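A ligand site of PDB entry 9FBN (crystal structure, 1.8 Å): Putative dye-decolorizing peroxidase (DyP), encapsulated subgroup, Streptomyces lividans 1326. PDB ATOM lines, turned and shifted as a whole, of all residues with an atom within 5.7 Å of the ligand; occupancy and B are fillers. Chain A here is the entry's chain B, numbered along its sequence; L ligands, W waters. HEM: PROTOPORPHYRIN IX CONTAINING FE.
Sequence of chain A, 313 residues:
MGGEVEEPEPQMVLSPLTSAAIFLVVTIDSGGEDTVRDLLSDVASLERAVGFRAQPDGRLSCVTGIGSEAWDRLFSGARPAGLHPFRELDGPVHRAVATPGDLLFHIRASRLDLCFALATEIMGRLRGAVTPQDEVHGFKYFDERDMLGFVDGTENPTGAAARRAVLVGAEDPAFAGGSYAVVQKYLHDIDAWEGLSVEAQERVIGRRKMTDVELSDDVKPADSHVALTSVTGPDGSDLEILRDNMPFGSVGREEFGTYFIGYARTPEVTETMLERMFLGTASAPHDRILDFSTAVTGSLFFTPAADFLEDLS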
ATOM      1  N   ASP A 146     -15.518 -11.958  28.169  1.00  0.00           N
ATOM      2  CA  ASP A 146     -14.955 -13.281  28.470  1.00  0.00           C
ATOM      3  C   ASP A 146     -13.532 -13.314  27.920  1.00  0.00           C
ATOM      4  O   ASP A 146     -12.971 -12.295  27.470  1.00  0.00           O
ATOM      5  CB  ASP A 146     -15.850 -14.408  27.998  1.00  0.00           C
ATOM      6  CG  ASP A 146     -16.207 -14.398  26.513  1.00  0.00           C
ATOM      7  OD1 ASP A 146     -15.425 -13.762  25.731  1.00  0.00           O
ATOM      8  OD2 ASP A 146     -17.263 -15.075  26.155  1.00  0.00           O
ATOM      9  N   LEU A 148     -12.421 -14.597  25.241  1.00  0.00           N
ATOM     10  CA  LEU A 148     -12.386 -14.330  23.803  1.00  0.00           C
ATOM     11  C   LEU A 148     -12.604 -12.856  23.458  1.00  0.00           C
ATOM     12  O   LEU A 148     -12.523 -12.510  22.252  1.00  0.00           O
ATOM     13  CB  LEU A 148     -13.453 -15.211  23.148  1.00  0.00           C
ATOM     14  CG  LEU A 148     -13.287 -16.743  23.337  1.00  0.00           C
ATOM     15  CD1 LEU A 148     -14.300 -17.583  22.597  1.00  0.00           C
ATOM     16  CD2 LEU A 148     -11.864 -17.308  22.981  1.00  0.00           C
ATOM     17  N   PHE A 150     -15.388 -10.944  23.932  1.00  0.00           N
ATOM     18  CA  PHE A 150     -16.799 -10.636  23.621  1.00  0.00           C
ATOM     19  C   PHE A 150     -17.612 -10.520  24.889  1.00  0.00           C
ATOM     20  O   PHE A 150     -17.338 -11.217  25.865  1.00  0.00           O
ATOM     21  CB  PHE A 150     -17.406 -11.764  22.751  1.00  0.00           C
ATOM     22  CG  PHE A 150     -17.061 -11.696  21.271  1.00  0.00           C
ATOM     23  CD1 PHE A 150     -15.764 -11.893  20.803  1.00  0.00           C
ATOM     24  CD2 PHE A 150     -18.022 -11.333  20.351  1.00  0.00           C
ATOM     25  CE1 PHE A 150     -15.489 -11.793  19.442  1.00  0.00           C
ATOM     26  CE2 PHE A 150     -17.706 -11.120  19.016  1.00  0.00           C
ATOM     27  CZ  PHE A 150     -16.436 -11.323  18.560  1.00  0.00           C
ATOM     28  N   VAL A 151     -18.572  -9.556  24.916  1.00  0.00           N
ATOM     29  CA  VAL A 151     -19.492  -9.469  26.049  1.00  0.00           C
ATOM     30  C   VAL A 151     -20.173 -10.819  26.161  1.00  0.00           C
ATOM     31  O   VAL A 151     -20.633 -11.361  25.163  1.00  0.00           O
ATOM     32  CB  VAL A 151     -20.507  -8.342  25.832  1.00  0.00           C
ATOM     33  CG1 VAL A 151     -21.514  -8.317  26.960  1.00  0.00           C
ATOM     34  CG2 VAL A 151     -19.800  -7.039  25.597  1.00  0.00           C
ATOM     35  N   ASP A 152     -20.310 -11.314  27.386  1.00  0.00           N
ATOM     36  CA  ASP A 152     -20.873 -12.630  27.584  1.00  0.00           C
ATOM     37  C   ASP A 152     -21.978 -12.590  28.649  1.00  0.00           C
ATOM     38  O   ASP A 152     -21.665 -12.390  29.837  1.00  0.00           O
ATOM     39  CB  ASP A 152     -19.710 -13.508  28.031  1.00  0.00           C
ATOM     40  CG  ASP A 152     -19.916 -15.013  28.019  1.00  0.00           C
ATOM     41  OD1 ASP A 152     -21.019 -15.425  28.279  1.00  0.00           O
ATOM     42  OD2 ASP A 152     -18.932 -15.700  27.711  1.00  0.00           O
ATOM     43  N   GLY A 153     -23.207 -12.837  28.237  1.00  0.00           N
ATOM     44  CA  GLY A 153     -24.376 -12.972  29.104  1.00  0.00           C
ATOM     45  C   GLY A 153     -25.590 -12.111  28.656  1.00  0.00           C
ATOM     46  O   GLY A 153     -26.661 -12.178  29.243  1.00  0.00           O
ATOM     47  N   THR A 154     -25.435 -11.432  27.528  1.00  0.00           N
ATOM     48  CA  THR A 154     -26.349 -10.458  26.961  1.00  0.00           C
ATOM     49  C   THR A 154     -27.753 -11.017  26.849  1.00  0.00           C
ATOM     50  O   THR A 154     -28.731 -10.405  27.285  1.00  0.00           O
ATOM     51  CB  THR A 154     -25.785 -10.080  25.598  1.00  0.00           C
ATOM     52  OG1 THR A 154     -24.432  -9.660  25.852  1.00  0.00           O
ATOM     53  CG2 THR A 154     -26.672  -9.066  24.935  1.00  0.00           C
ATOM     54  N   GLU A 155     -27.863 -12.248  26.330  1.00  0.00           N
ATOM     55  CA  GLU A 155     -29.149 -12.830  26.011  1.00  0.00           C
ATOM     56  C   GLU A 155     -29.732 -13.690  27.102  1.00  0.00           C
ATOM     57  O   GLU A 155     -30.815 -14.257  26.903  1.00  0.00           O
ATOM     58  CB  GLU A 155     -29.224 -13.511  24.631  1.00  0.00           C
ATOM     59  CG  GLU A 155     -29.131 -12.437  23.558  1.00  0.00           C
ATOM     60  CD  GLU A 155     -30.377 -11.531  23.428  1.00  0.00           C
ATOM     61  OE1 GLU A 155     -31.451 -12.192  23.273  1.00  0.00           O
ATOM     62  OE2 GLU A 155     -30.295 -10.229  23.479  1.00  0.00           O
ATOM     63  N   ASN A 156     -29.121 -13.661  28.293  1.00  0.00           N
ATOM     64  CA  ASN A 156     -29.746 -14.386  29.365  1.00  0.00           C
ATOM     65  C   ASN A 156     -31.153 -13.833  29.621  1.00  0.00           C
ATOM     66  O   ASN A 156     -31.376 -12.600  29.623  1.00  0.00           O
ATOM     67  CB  ASN A 156     -29.009 -14.295  30.701  1.00  0.00           C
ATOM     68  CG  ASN A 156     -27.887 -15.285  30.884  1.00  0.00           C
ATOM     69  OD1 ASN A 156     -27.946 -16.448  30.445  1.00  0.00           O
ATOM     70  ND2 ASN A 156     -26.859 -14.841  31.591  1.00  0.00           N
ATOM     71  N   GLN A 184     -18.998 -27.400  32.164  1.00  0.00           N
ATOM     72  CA  GLN A 184     -17.924 -27.801  31.264  1.00  0.00           C
ATOM     73  C   GLN A 184     -16.805 -26.815  31.398  1.00  0.00           C
ATOM     74  O   GLN A 184     -17.007 -25.638  31.232  1.00  0.00           O
ATOM     75  CB  GLN A 184     -18.269 -27.808  29.770  1.00  0.00           C
ATOM     76  CG  GLN A 184     -19.374 -28.781  29.442  1.00  0.00           C
ATOM     77  CD  GLN A 184     -19.740 -28.753  27.999  1.00  0.00           C
ATOM     78  OE1 GLN A 184     -20.177 -27.742  27.448  1.00  0.00           O
ATOM     79  NE2 GLN A 184     -19.394 -29.826  27.306  1.00  0.00           N
ATOM     80  N   TYR A 186     -13.653 -25.265  29.721  1.00  0.00           N
ATOM     81  CA  TYR A 186     -13.038 -25.212  28.424  1.00  0.00           C
ATOM     82  C   TYR A 186     -11.696 -24.481  28.489  1.00  0.00           C
ATOM     83  O   TYR A 186     -11.628 -23.359  29.084  1.00  0.00           O
ATOM     84  CB  TYR A 186     -13.944 -24.436  27.473  1.00  0.00           C
ATOM     85  CG  TYR A 186     -15.198 -25.101  26.975  1.00  0.00           C
ATOM     86  CD1 TYR A 186     -16.422 -25.015  27.655  1.00  0.00           C
ATOM     87  CD2 TYR A 186     -15.182 -25.792  25.753  1.00  0.00           C
ATOM     88  CE1 TYR A 186     -17.563 -25.683  27.182  1.00  0.00           C
ATOM     89  CE2 TYR A 186     -16.305 -26.455  25.271  1.00  0.00           C
ATOM     90  CZ  TYR A 186     -17.506 -26.382  25.972  1.00  0.00           C
ATOM     91  OH  TYR A 186     -18.616 -26.964  25.388  1.00  0.00           O
ATOM     92  N   HIS A 188      -9.022 -22.585  25.838  1.00  0.00           N
ATOM     93  CA  HIS A 188      -8.952 -21.944  24.540  1.00  0.00           C
ATOM     94  C   HIS A 188      -7.529 -22.046  23.976  1.00  0.00           C
ATOM     95  O   HIS A 188      -6.560 -21.981  24.744  1.00  0.00           O
ATOM     96  CB  HIS A 188      -9.359 -20.471  24.691  1.00  0.00           C
ATOM     97  CG  HIS A 188     -10.766 -20.373  25.157  1.00  0.00           C
ATOM     98  ND1 HIS A 188     -11.779 -20.898  24.414  1.00  0.00           N
ATOM     99  CD2 HIS A 188     -11.346 -19.746  26.195  1.00  0.00           C
ATOM    100  CE1 HIS A 188     -12.943 -20.624  25.004  1.00  0.00           C
ATOM    101  NE2 HIS A 188     -12.700 -19.929  26.104  1.00  0.00           N
ATOM    102  N   ILE A 205     -18.859 -15.999  16.545  1.00  0.00           N
ATOM    103  CA  ILE A 205     -19.803 -15.875  17.641  1.00  0.00           C
ATOM    104  C   ILE A 205     -21.222 -15.629  17.095  1.00  0.00           C
ATOM    105  O   ILE A 205     -22.191 -16.165  17.649  1.00  0.00           O
ATOM    106  CB  ILE A 205     -19.283 -14.691  18.496  1.00  0.00           C
ATOM    107  CG1 ILE A 205     -17.841 -15.007  19.084  1.00  0.00           C
ATOM    108  CG2 ILE A 205     -20.288 -14.308  19.573  1.00  0.00           C
ATOM    109  CD1 ILE A 205     -17.769 -16.239  19.932  1.00  0.00           C
ATOM    110  N   ARG A 207     -22.146 -12.050  16.848  1.00  0.00           N
ATOM    111  CA  ARG A 207     -22.409 -10.677  17.281  1.00  0.00           C
ATOM    112  C   ARG A 207     -21.238  -9.736  16.986  1.00  0.00           C
ATOM    113  O   ARG A 207     -20.142 -10.203  16.885  1.00  0.00           O
ATOM    114  CB  ARG A 207     -22.752 -10.643  18.771  1.00  0.00           C
ATOM    115  CG  ARG A 207     -23.747 -11.699  19.228  1.00  0.00           C
ATOM    116  CD  ARG A 207     -24.184 -11.643  20.666  1.00  0.00           C
ATOM    117  NE  ARG A 207     -24.837 -10.398  21.078  1.00  0.00           N
ATOM    118  CZ  ARG A 207     -26.175 -10.180  21.097  1.00  0.00           C
ATOM    119  NH1 ARG A 207     -26.658  -8.968  21.364  1.00  0.00           N
ATOM    120  NH2 ARG A 207     -26.993 -11.137  20.848  1.00  0.00           N
ATOM    121  N   ASP A 212     -21.567  -5.274  20.527  1.00  0.00           N
ATOM    122  CA  ASP A 212     -22.370  -6.431  20.907  1.00  0.00           C
ATOM    123  C   ASP A 212     -23.766  -6.400  20.316  1.00  0.00           C
ATOM    124  O   ASP A 212     -24.694  -6.918  20.899  1.00  0.00           O
ATOM    125  CB  ASP A 212     -22.434  -6.526  22.428  1.00  0.00           C
ATOM    126  CG  ASP A 212     -23.025  -7.756  23.108  1.00  0.00           C
ATOM    127  OD1 ASP A 212     -22.950  -8.849  22.552  1.00  0.00           O
ATOM    128  OD2 ASP A 212     -23.569  -7.595  24.224  1.00  0.00           O
ATOM    129  N   GLU A 214     -26.315  -8.047  17.650  1.00  0.00           N
ATOM    130  CA  GLU A 214     -26.387  -9.315  16.936  1.00  0.00           C
ATOM    131  C   GLU A 214     -26.271  -9.091  15.428  1.00  0.00           C
ATOM    132  O   GLU A 214     -26.719  -8.080  14.905  1.00  0.00           O
ATOM    133  CB  GLU A 214     -27.706  -9.987  17.324  1.00  0.00           C
ATOM    134  CG  GLU A 214     -27.930 -11.371  16.737  1.00  0.00           C
ATOM    135  CD  GLU A 214     -29.214 -12.041  17.132  1.00  0.00           C
ATOM    136  OE1 GLU A 214     -29.964 -11.465  17.925  1.00  0.00           O
ATOM    137  OE2 GLU A 214     -29.400 -13.209  16.730  1.00  0.00           O
ATOM    138  N   HIS A 225     -21.972 -19.634  16.800  1.00  0.00           N
ATOM    139  CA  HIS A 225     -22.418 -19.999  18.132  1.00  0.00           C
ATOM    140  C   HIS A 225     -23.855 -19.567  18.434  1.00  0.00           C
ATOM    141  O   HIS A 225     -24.622 -20.333  18.967  1.00  0.00           O
ATOM    142  CB  HIS A 225     -21.433 -19.396  19.118  1.00  0.00           C
ATOM    143  CG  HIS A 225     -21.675 -19.873  20.498  1.00  0.00           C
ATOM    144  ND1 HIS A 225     -21.636 -21.198  20.824  1.00  0.00           N
ATOM    145  CD2 HIS A 225     -21.833 -19.193  21.617  1.00  0.00           C
ATOM    146  CE1 HIS A 225     -21.928 -21.312  22.112  1.00  0.00           C
ATOM    147  NE2 HIS A 225     -22.032 -20.061  22.613  1.00  0.00           N
ATOM    148  N   VAL A 226     -24.191 -18.294  18.193  1.00  0.00           N
ATOM    149  CA  VAL A 226     -25.540 -17.800  18.500  1.00  0.00           C
ATOM    150  C   VAL A 226     -26.594 -18.546  17.664  1.00  0.00           C
ATOM    151  O   VAL A 226     -27.666 -18.848  18.191  1.00  0.00           O
ATOM    152  CB  VAL A 226     -25.650 -16.285  18.326  1.00  0.00           C
ATOM    153  CG1 VAL A 226     -27.109 -15.821  18.228  1.00  0.00           C
ATOM    154  CG2 VAL A 226     -24.919 -15.570  19.434  1.00  0.00           C
ATOM    155  N   THR A 229     -27.164 -22.178  19.131  1.00  0.00           N
ATOM    156  CA  THR A 229     -27.655 -22.367  20.487  1.00  0.00           C
ATOM    157  C   THR A 229     -29.014 -21.721  20.570  1.00  0.00           C
ATOM    158  O   THR A 229     -29.585 -21.587  21.659  1.00  0.00           O
ATOM    159  CB  THR A 229     -26.658 -21.857  21.549  1.00  0.00           C
ATOM    160  OG1 THR A 229     -26.275 -20.520  21.306  1.00  0.00           O
ATOM    161  CG2 THR A 229     -25.373 -22.656  21.570  1.00  0.00           C
ATOM    162  N   SER A 230     -29.502 -21.302  19.402  1.00  0.00           N
ATOM    163  CA  SER A 230     -30.841 -20.748  19.299  1.00  0.00           C
ATOM    164  C   SER A 230     -31.771 -21.905  18.961  1.00  0.00           C
ATOM    165  O   SER A 230     -31.617 -22.508  17.905  1.00  0.00           O
ATOM    166  CB  SER A 230     -30.905 -19.652  18.261  1.00  0.00           C
ATOM    167  OG  SER A 230     -30.280 -18.491  18.746  1.00  0.00           O
ATOM    168  N   ILE A 241     -31.785 -20.833  28.332  1.00  0.00           N
ATOM    169  CA  ILE A 241     -31.099 -21.194  29.576  1.00  0.00           C
ATOM    170  C   ILE A 241     -30.507 -19.965  30.259  1.00  0.00           C
ATOM    171  O   ILE A 241     -30.457 -18.878  29.694  1.00  0.00           O
ATOM    172  CB  ILE A 241     -30.038 -22.280  29.351  1.00  0.00           C
ATOM    173  CG1 ILE A 241     -28.895 -21.820  28.428  1.00  0.00           C
ATOM    174  CG2 ILE A 241     -30.647 -23.565  28.833  1.00  0.00           C
ATOM    175  CD1 ILE A 241     -27.746 -22.775  28.381  1.00  0.00           C
ATOM    176  N   ARG A 243     -27.043 -18.596  31.958  1.00  0.00           N
ATOM    177  CA  ARG A 243     -25.601 -18.845  31.985  1.00  0.00           C
ATOM    178  C   ARG A 243     -24.951 -17.932  33.014  1.00  0.00           C
ATOM    179  O   ARG A 243     -25.360 -16.770  33.192  1.00  0.00           O
ATOM    180  CB  ARG A 243     -25.028 -18.709  30.556  1.00  0.00           C
ATOM    181  CG  ARG A 243     -25.485 -19.823  29.629  1.00  0.00           C
ATOM    182  CD  ARG A 243     -25.347 -19.512  28.118  1.00  0.00           C
ATOM    183  NE  ARG A 243     -26.041 -18.286  27.689  1.00  0.00           N
ATOM    184  CZ  ARG A 243     -25.497 -17.118  27.413  1.00  0.00           C
ATOM    185  NH1 ARG A 243     -24.202 -16.946  27.204  1.00  0.00           N
ATOM    186  NH2 ARG A 243     -26.279 -16.121  27.170  1.00  0.00           N
ATOM    187  N   ASN A 245     -21.030 -17.791  32.752  1.00  0.00           N
ATOM    188  CA  ASN A 245     -19.714 -18.243  32.312  1.00  0.00           C
ATOM    189  C   ASN A 245     -18.618 -17.370  32.929  1.00  0.00           C
ATOM    190  O   ASN A 245     -18.713 -16.136  32.994  1.00  0.00           O
ATOM    191  CB  ASN A 245     -19.548 -18.062  30.794  1.00  0.00           C
ATOM    192  CG  ASN A 245     -20.450 -18.901  29.945  1.00  0.00           C
ATOM    193  OD1 ASN A 245     -21.037 -19.882  30.438  1.00  0.00           O
ATOM    194  ND2 ASN A 245     -20.639 -18.502  28.687  1.00  0.00           N
ATOM    195  N   THR A 258     -12.589 -20.784  29.717  1.00  0.00           N
ATOM    196  CA  THR A 258     -13.953 -20.372  30.047  1.00  0.00           C
ATOM    197  C   THR A 258     -14.579 -21.515  30.852  1.00  0.00           C
ATOM    198  O   THR A 258     -14.644 -22.651  30.387  1.00  0.00           O
ATOM    199  CB  THR A 258     -14.865 -20.061  28.844  1.00  0.00           C
ATOM    200  OG1 THR A 258     -14.314 -19.007  28.102  1.00  0.00           O
ATOM    201  CG2 THR A 258     -16.267 -19.666  29.336  1.00  0.00           C
ATOM    202  N   PHE A 260     -17.877 -23.018  31.819  1.00  0.00           N
ATOM    203  CA  PHE A 260     -19.270 -22.971  31.400  1.00  0.00           C
ATOM    204  C   PHE A 260     -20.165 -23.559  32.493  1.00  0.00           C
ATOM    205  O   PHE A 260     -19.967 -24.656  32.903  1.00  0.00           O
ATOM    206  CB  PHE A 260     -19.524 -23.700  30.073  1.00  0.00           C
ATOM    207  CG  PHE A 260     -21.001 -23.840  29.767  1.00  0.00           C
ATOM    208  CD1 PHE A 260     -21.702 -22.795  29.192  1.00  0.00           C
ATOM    209  CD2 PHE A 260     -21.697 -24.997  30.084  1.00  0.00           C
ATOM    210  CE1 PHE A 260     -23.076 -22.929  28.951  1.00  0.00           C
ATOM    211  CE2 PHE A 260     -23.039 -25.126  29.841  1.00  0.00           C
ATOM    212  CZ  PHE A 260     -23.726 -24.090  29.268  1.00  0.00           C
ATOM    213  N   THR A 270     -30.611 -27.935  27.559  1.00  0.00           N
ATOM    214  CA  THR A 270     -29.154 -27.788  27.481  1.00  0.00           C
ATOM    215  C   THR A 270     -28.487 -28.868  26.622  1.00  0.00           C
ATOM    216  O   THR A 270     -27.503 -28.655  25.837  1.00  0.00           O
ATOM    217  CB  THR A 270     -28.567 -27.839  28.881  1.00  0.00           C
ATOM    218  OG1 THR A 270     -29.256 -26.957  29.731  1.00  0.00           O
ATOM    219  CG2 THR A 270     -27.100 -27.476  28.820  1.00  0.00           C
ATOM    220  N   MET A 273     -28.923 -28.087  22.856  1.00  0.00           N
ATOM    221  CA  MET A 273     -27.887 -27.166  22.418  1.00  0.00           C
ATOM    222  C   MET A 273     -26.523 -27.851  22.245  1.00  0.00           C
ATOM    223  O   MET A 273     -25.854 -27.553  21.267  1.00  0.00           O
ATOM    224  CB  MET A 273     -27.744 -25.969  23.388  1.00  0.00           C
ATOM    225  CG  MET A 273     -29.005 -25.199  23.642  1.00  0.00           C
ATOM    226  SD  MET A 273     -28.953 -23.930  24.963  1.00  0.00           S
ATOM    227  CE  MET A 273     -30.446 -23.026  24.566  1.00  0.00           C
ATOM    228  N   LEU A 274     -26.045 -28.618  23.267  1.00  0.00           N
ATOM    229  CA  LEU A 274     -24.851 -29.429  23.171  1.00  0.00           C
ATOM    230  C   LEU A 274     -24.869 -30.314  21.914  1.00  0.00           C
ATOM    231  O   LEU A 274     -23.852 -30.401  21.219  1.00  0.00           O
ATOM    232  CB  LEU A 274     -24.620 -30.244  24.448  1.00  0.00           C
ATOM    233  CG  LEU A 274     -24.162 -29.385  25.625  1.00  0.00           C
ATOM    234  CD1 LEU A 274     -24.188 -30.202  26.899  1.00  0.00           C
ATOM    235  CD2 LEU A 274     -22.771 -28.750  25.409  1.00  0.00           C
ATOM    236  N   MET A 277     -24.173 -28.140  18.912  1.00  0.00           N
ATOM    237  CA  MET A 277     -22.801 -27.655  18.933  1.00  0.00           C
ATOM    238  C   MET A 277     -21.849 -28.729  18.380  1.00  0.00           C
ATOM    239  O   MET A 277     -20.956 -28.425  17.566  1.00  0.00           O
ATOM    240  CB  MET A 277     -22.399 -27.201  20.346  1.00  0.00           C
ATOM    241  CG  MET A 277     -23.050 -25.806  20.665  1.00  0.00           C
ATOM    242  SD  MET A 277     -22.609 -25.358  22.351  1.00  0.00           S
ATOM    243  CE  MET A 277     -20.807 -25.274  22.287  1.00  0.00           C
ATOM    244  N   ILE A 289     -17.177 -22.130  17.444  1.00  0.00           N
ATOM    245  CA  ILE A 289     -16.486 -21.839  18.709  1.00  0.00           C
ATOM    246  C   ILE A 289     -15.632 -23.016  19.150  1.00  0.00           C
ATOM    247  O   ILE A 289     -14.636 -22.839  19.862  1.00  0.00           O
ATOM    248  CB  ILE A 289     -17.475 -21.330  19.793  1.00  0.00           C
ATOM    249  CG1 ILE A 289     -16.772 -20.346  20.778  1.00  0.00           C
ATOM    250  CG2 ILE A 289     -18.127 -22.474  20.509  1.00  0.00           C
ATOM    251  CD1 ILE A 289     -17.718 -19.578  21.693  1.00  0.00           C
ATOM    252  N   SER A 293     -11.774 -23.963  21.149  1.00  0.00           N
ATOM    253  CA  SER A 293     -12.272 -24.275  22.494  1.00  0.00           C
ATOM    254  C   SER A 293     -12.342 -25.786  22.720  1.00  0.00           C
ATOM    255  O   SER A 293     -13.032 -26.501  22.022  1.00  0.00           O
ATOM    256  CB  SER A 293     -13.678 -23.637  22.778  1.00  0.00           C
ATOM    257  OG  SER A 293     -13.726 -22.218  22.487  1.00  0.00           O
HETATM  258  CHA HEM L   1     -24.322 -16.860  23.807  1.00  0.00           C
HETATM  259  CHB HEM L   1     -19.639 -17.362  24.783  1.00  0.00           C
HETATM  260  CHC HEM L   1     -20.258 -22.051  25.581  1.00  0.00           C
HETATM  261  CHD HEM L   1     -24.990 -21.476  25.082  1.00  0.00           C
HETATM  262  C1A HEM L   1     -22.995 -16.615  23.924  1.00  0.00           C
HETATM  263  C2A HEM L   1     -22.395 -15.369  23.694  1.00  0.00           C
HETATM  264  C3A HEM L   1     -21.057 -15.503  23.907  1.00  0.00           C
HETATM  265  C4A HEM L   1     -20.884 -16.808  24.376  1.00  0.00           C
HETATM  266  CMA HEM L   1     -20.000 -14.451  23.723  1.00  0.00           C
HETATM  267  CAA HEM L   1     -23.028 -14.160  23.086  1.00  0.00           C
HETATM  268  CBA HEM L   1     -23.505 -13.086  24.100  1.00  0.00           C
HETATM  269  CGA HEM L   1     -24.486 -13.724  25.066  1.00  0.00           C
HETATM  270  O1A HEM L   1     -24.157 -14.116  26.215  1.00  0.00           O
HETATM  271  O2A HEM L   1     -25.694 -13.805  24.747  1.00  0.00           O
HETATM  272  C1B HEM L   1     -19.399 -18.737  25.082  1.00  0.00           C
HETATM  273  C2B HEM L   1     -18.089 -19.342  25.402  1.00  0.00           C
HETATM  274  C3B HEM L   1     -18.271 -20.665  25.654  1.00  0.00           C
HETATM  275  C4B HEM L   1     -19.708 -20.826  25.404  1.00  0.00           C
HETATM  276  CMB HEM L   1     -16.742 -18.623  25.473  1.00  0.00           C
HETATM  277  CAB HEM L   1     -17.547 -21.918  25.849  1.00  0.00           C
HETATM  278  CBB HEM L   1     -16.591 -22.269  25.094  1.00  0.00           C
HETATM  279  C1C HEM L   1     -21.630 -22.313  25.583  1.00  0.00           C
HETATM  280  C2C HEM L   1     -22.219 -23.597  25.687  1.00  0.00           C
HETATM  281  C3C HEM L   1     -23.579 -23.466  25.552  1.00  0.00           C
HETATM  282  C4C HEM L   1     -23.764 -22.034  25.340  1.00  0.00           C
HETATM  283  CMC HEM L   1     -21.550 -24.897  26.067  1.00  0.00           C
HETATM  284  CAC HEM L   1     -24.692 -24.416  25.716  1.00  0.00           C
HETATM  285  CBC HEM L   1     -24.827 -25.711  25.962  1.00  0.00           C
HETATM  286  C1D HEM L   1     -25.196 -20.152  24.678  1.00  0.00           C
HETATM  287  C2D HEM L   1     -26.571 -19.606  24.432  1.00  0.00           C
HETATM  288  C3D HEM L   1     -26.400 -18.329  24.154  1.00  0.00           C
HETATM  289  C4D HEM L   1     -24.887 -18.131  24.105  1.00  0.00           C
HETATM  290  CMD HEM L   1     -27.815 -20.379  24.572  1.00  0.00           C
HETATM  291  CAD HEM L   1     -27.440 -17.387  23.719  1.00  0.00           C
HETATM  292  CBD HEM L   1     -27.830 -17.474  22.230  1.00  0.00           C
HETATM  293  CGD HEM L   1     -28.925 -16.444  21.872  1.00  0.00           C
HETATM  294  O1D HEM L   1     -28.675 -15.235  21.531  1.00  0.00           O
HETATM  295  O2D HEM L   1     -30.102 -16.737  22.159  1.00  0.00           O
HETATM  296  NA  HEM L   1     -22.118 -17.434  24.519  1.00  0.00           N
HETATM  297  NB  HEM L   1     -20.340 -19.613  25.168  1.00  0.00           N
HETATM  298  NC  HEM L   1     -22.559 -21.400  25.156  1.00  0.00           N
HETATM  299  ND  HEM L   1     -24.254 -19.264  24.470  1.00  0.00           N
HETATM  300 FE   HEM L   1     -22.347 -19.450  24.761  1.00  0.00          FE
HETATM  301  O   HOH W   1     -30.925 -19.360  23.246  1.00  0.00           O
HETATM  302  O   HOH W   2     -26.373 -14.009  22.041  1.00  0.00           O
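Merely in contact with the ligand: Thr 229, Phe 260, Asp 152, Gln 184, Val 151, Asp 146, Thr 258, Tyr 186, Arg 207, Val 226, Asn 245, Leu 274, Met 273, Ile 289, Met 277, Ser 230, Phe 150, Ser 293, Leu 148 and Thr 270. Hydrophobic or aromatic side chains that line the ligand: Leu 148, Phe 150, Tyr 186, His 225, Val 226, Phe 260, Met 273, Leu 274, Met 277 and Ile 289. Along chain A the residues within 4 Å of the ligand span positions 146 to 293. The nearest printed residue that does not touch the ligand is His 188 (4.003 Å).
The guanidinium group (NH1) of Arg 243 lies within salt-bridge range of the side-chain carboxylate (OD1) of Asp 152, 3.7 Å away. N of Arg 243 lies within hydrogen-bond range of OD1 of Asn 156, at 2.8 Å. OD1 of Asp 152 sits at hydrogen-bond distance from ND2 of Asn 245. The backbone NH (N) of Phe 150 lies within hydrogen-bond range of the side-chain carboxylate (OD1) of Asp 146 (3.3 Å). The side-chain carboxylate of Asp 146 lies within hydrogen-bond range of the backbone NH of Leu 148 (3.2 Å). OG1 of Thr 258 lies within hydrogen-bond range of NE2 of His 188 (2.7 Å). The backbone carbonyl oxygen of Val 226 sits at hydrogen-bond distance from the side-chain hydroxyl of Ser 230, at 2.7 Å. The side-chain hydroxyl (OG) of Ser 293 lies within hydrogen-bond range of a ring nitrogen (ND1) of His 188 (3.0 Å).
Water W2 bridges O1D of the ligand (2.7 Å) and NH2 of Arg 207 (3.2 Å). Water W1 lies within hydrogen-bond range of O2D of the ligand (3.0 Å) and O of Thr 229 (3.0 Å).
An iron atom (FE) of the ligand is bound by a ring nitrogen (NE2) of His 225 (2.3 Å). N of Gly 153 is in hydrogen-bond range of O1A of the ligand, 2.6 Å away. The guanidinium group (NH1) of Arg 243 is in salt-bridge range of an oxygen (O1A) of the ligand (3.0 Å). The backbone NH (N) of Glu 155 lies within hydrogen-bond range of an oxygen (O2A) of the ligand, at 3.1 Å. The backbone NH (N) of Thr 154 lies within hydrogen-bond range of an oxygen (O1A) of the ligand, at 3.2 Å.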
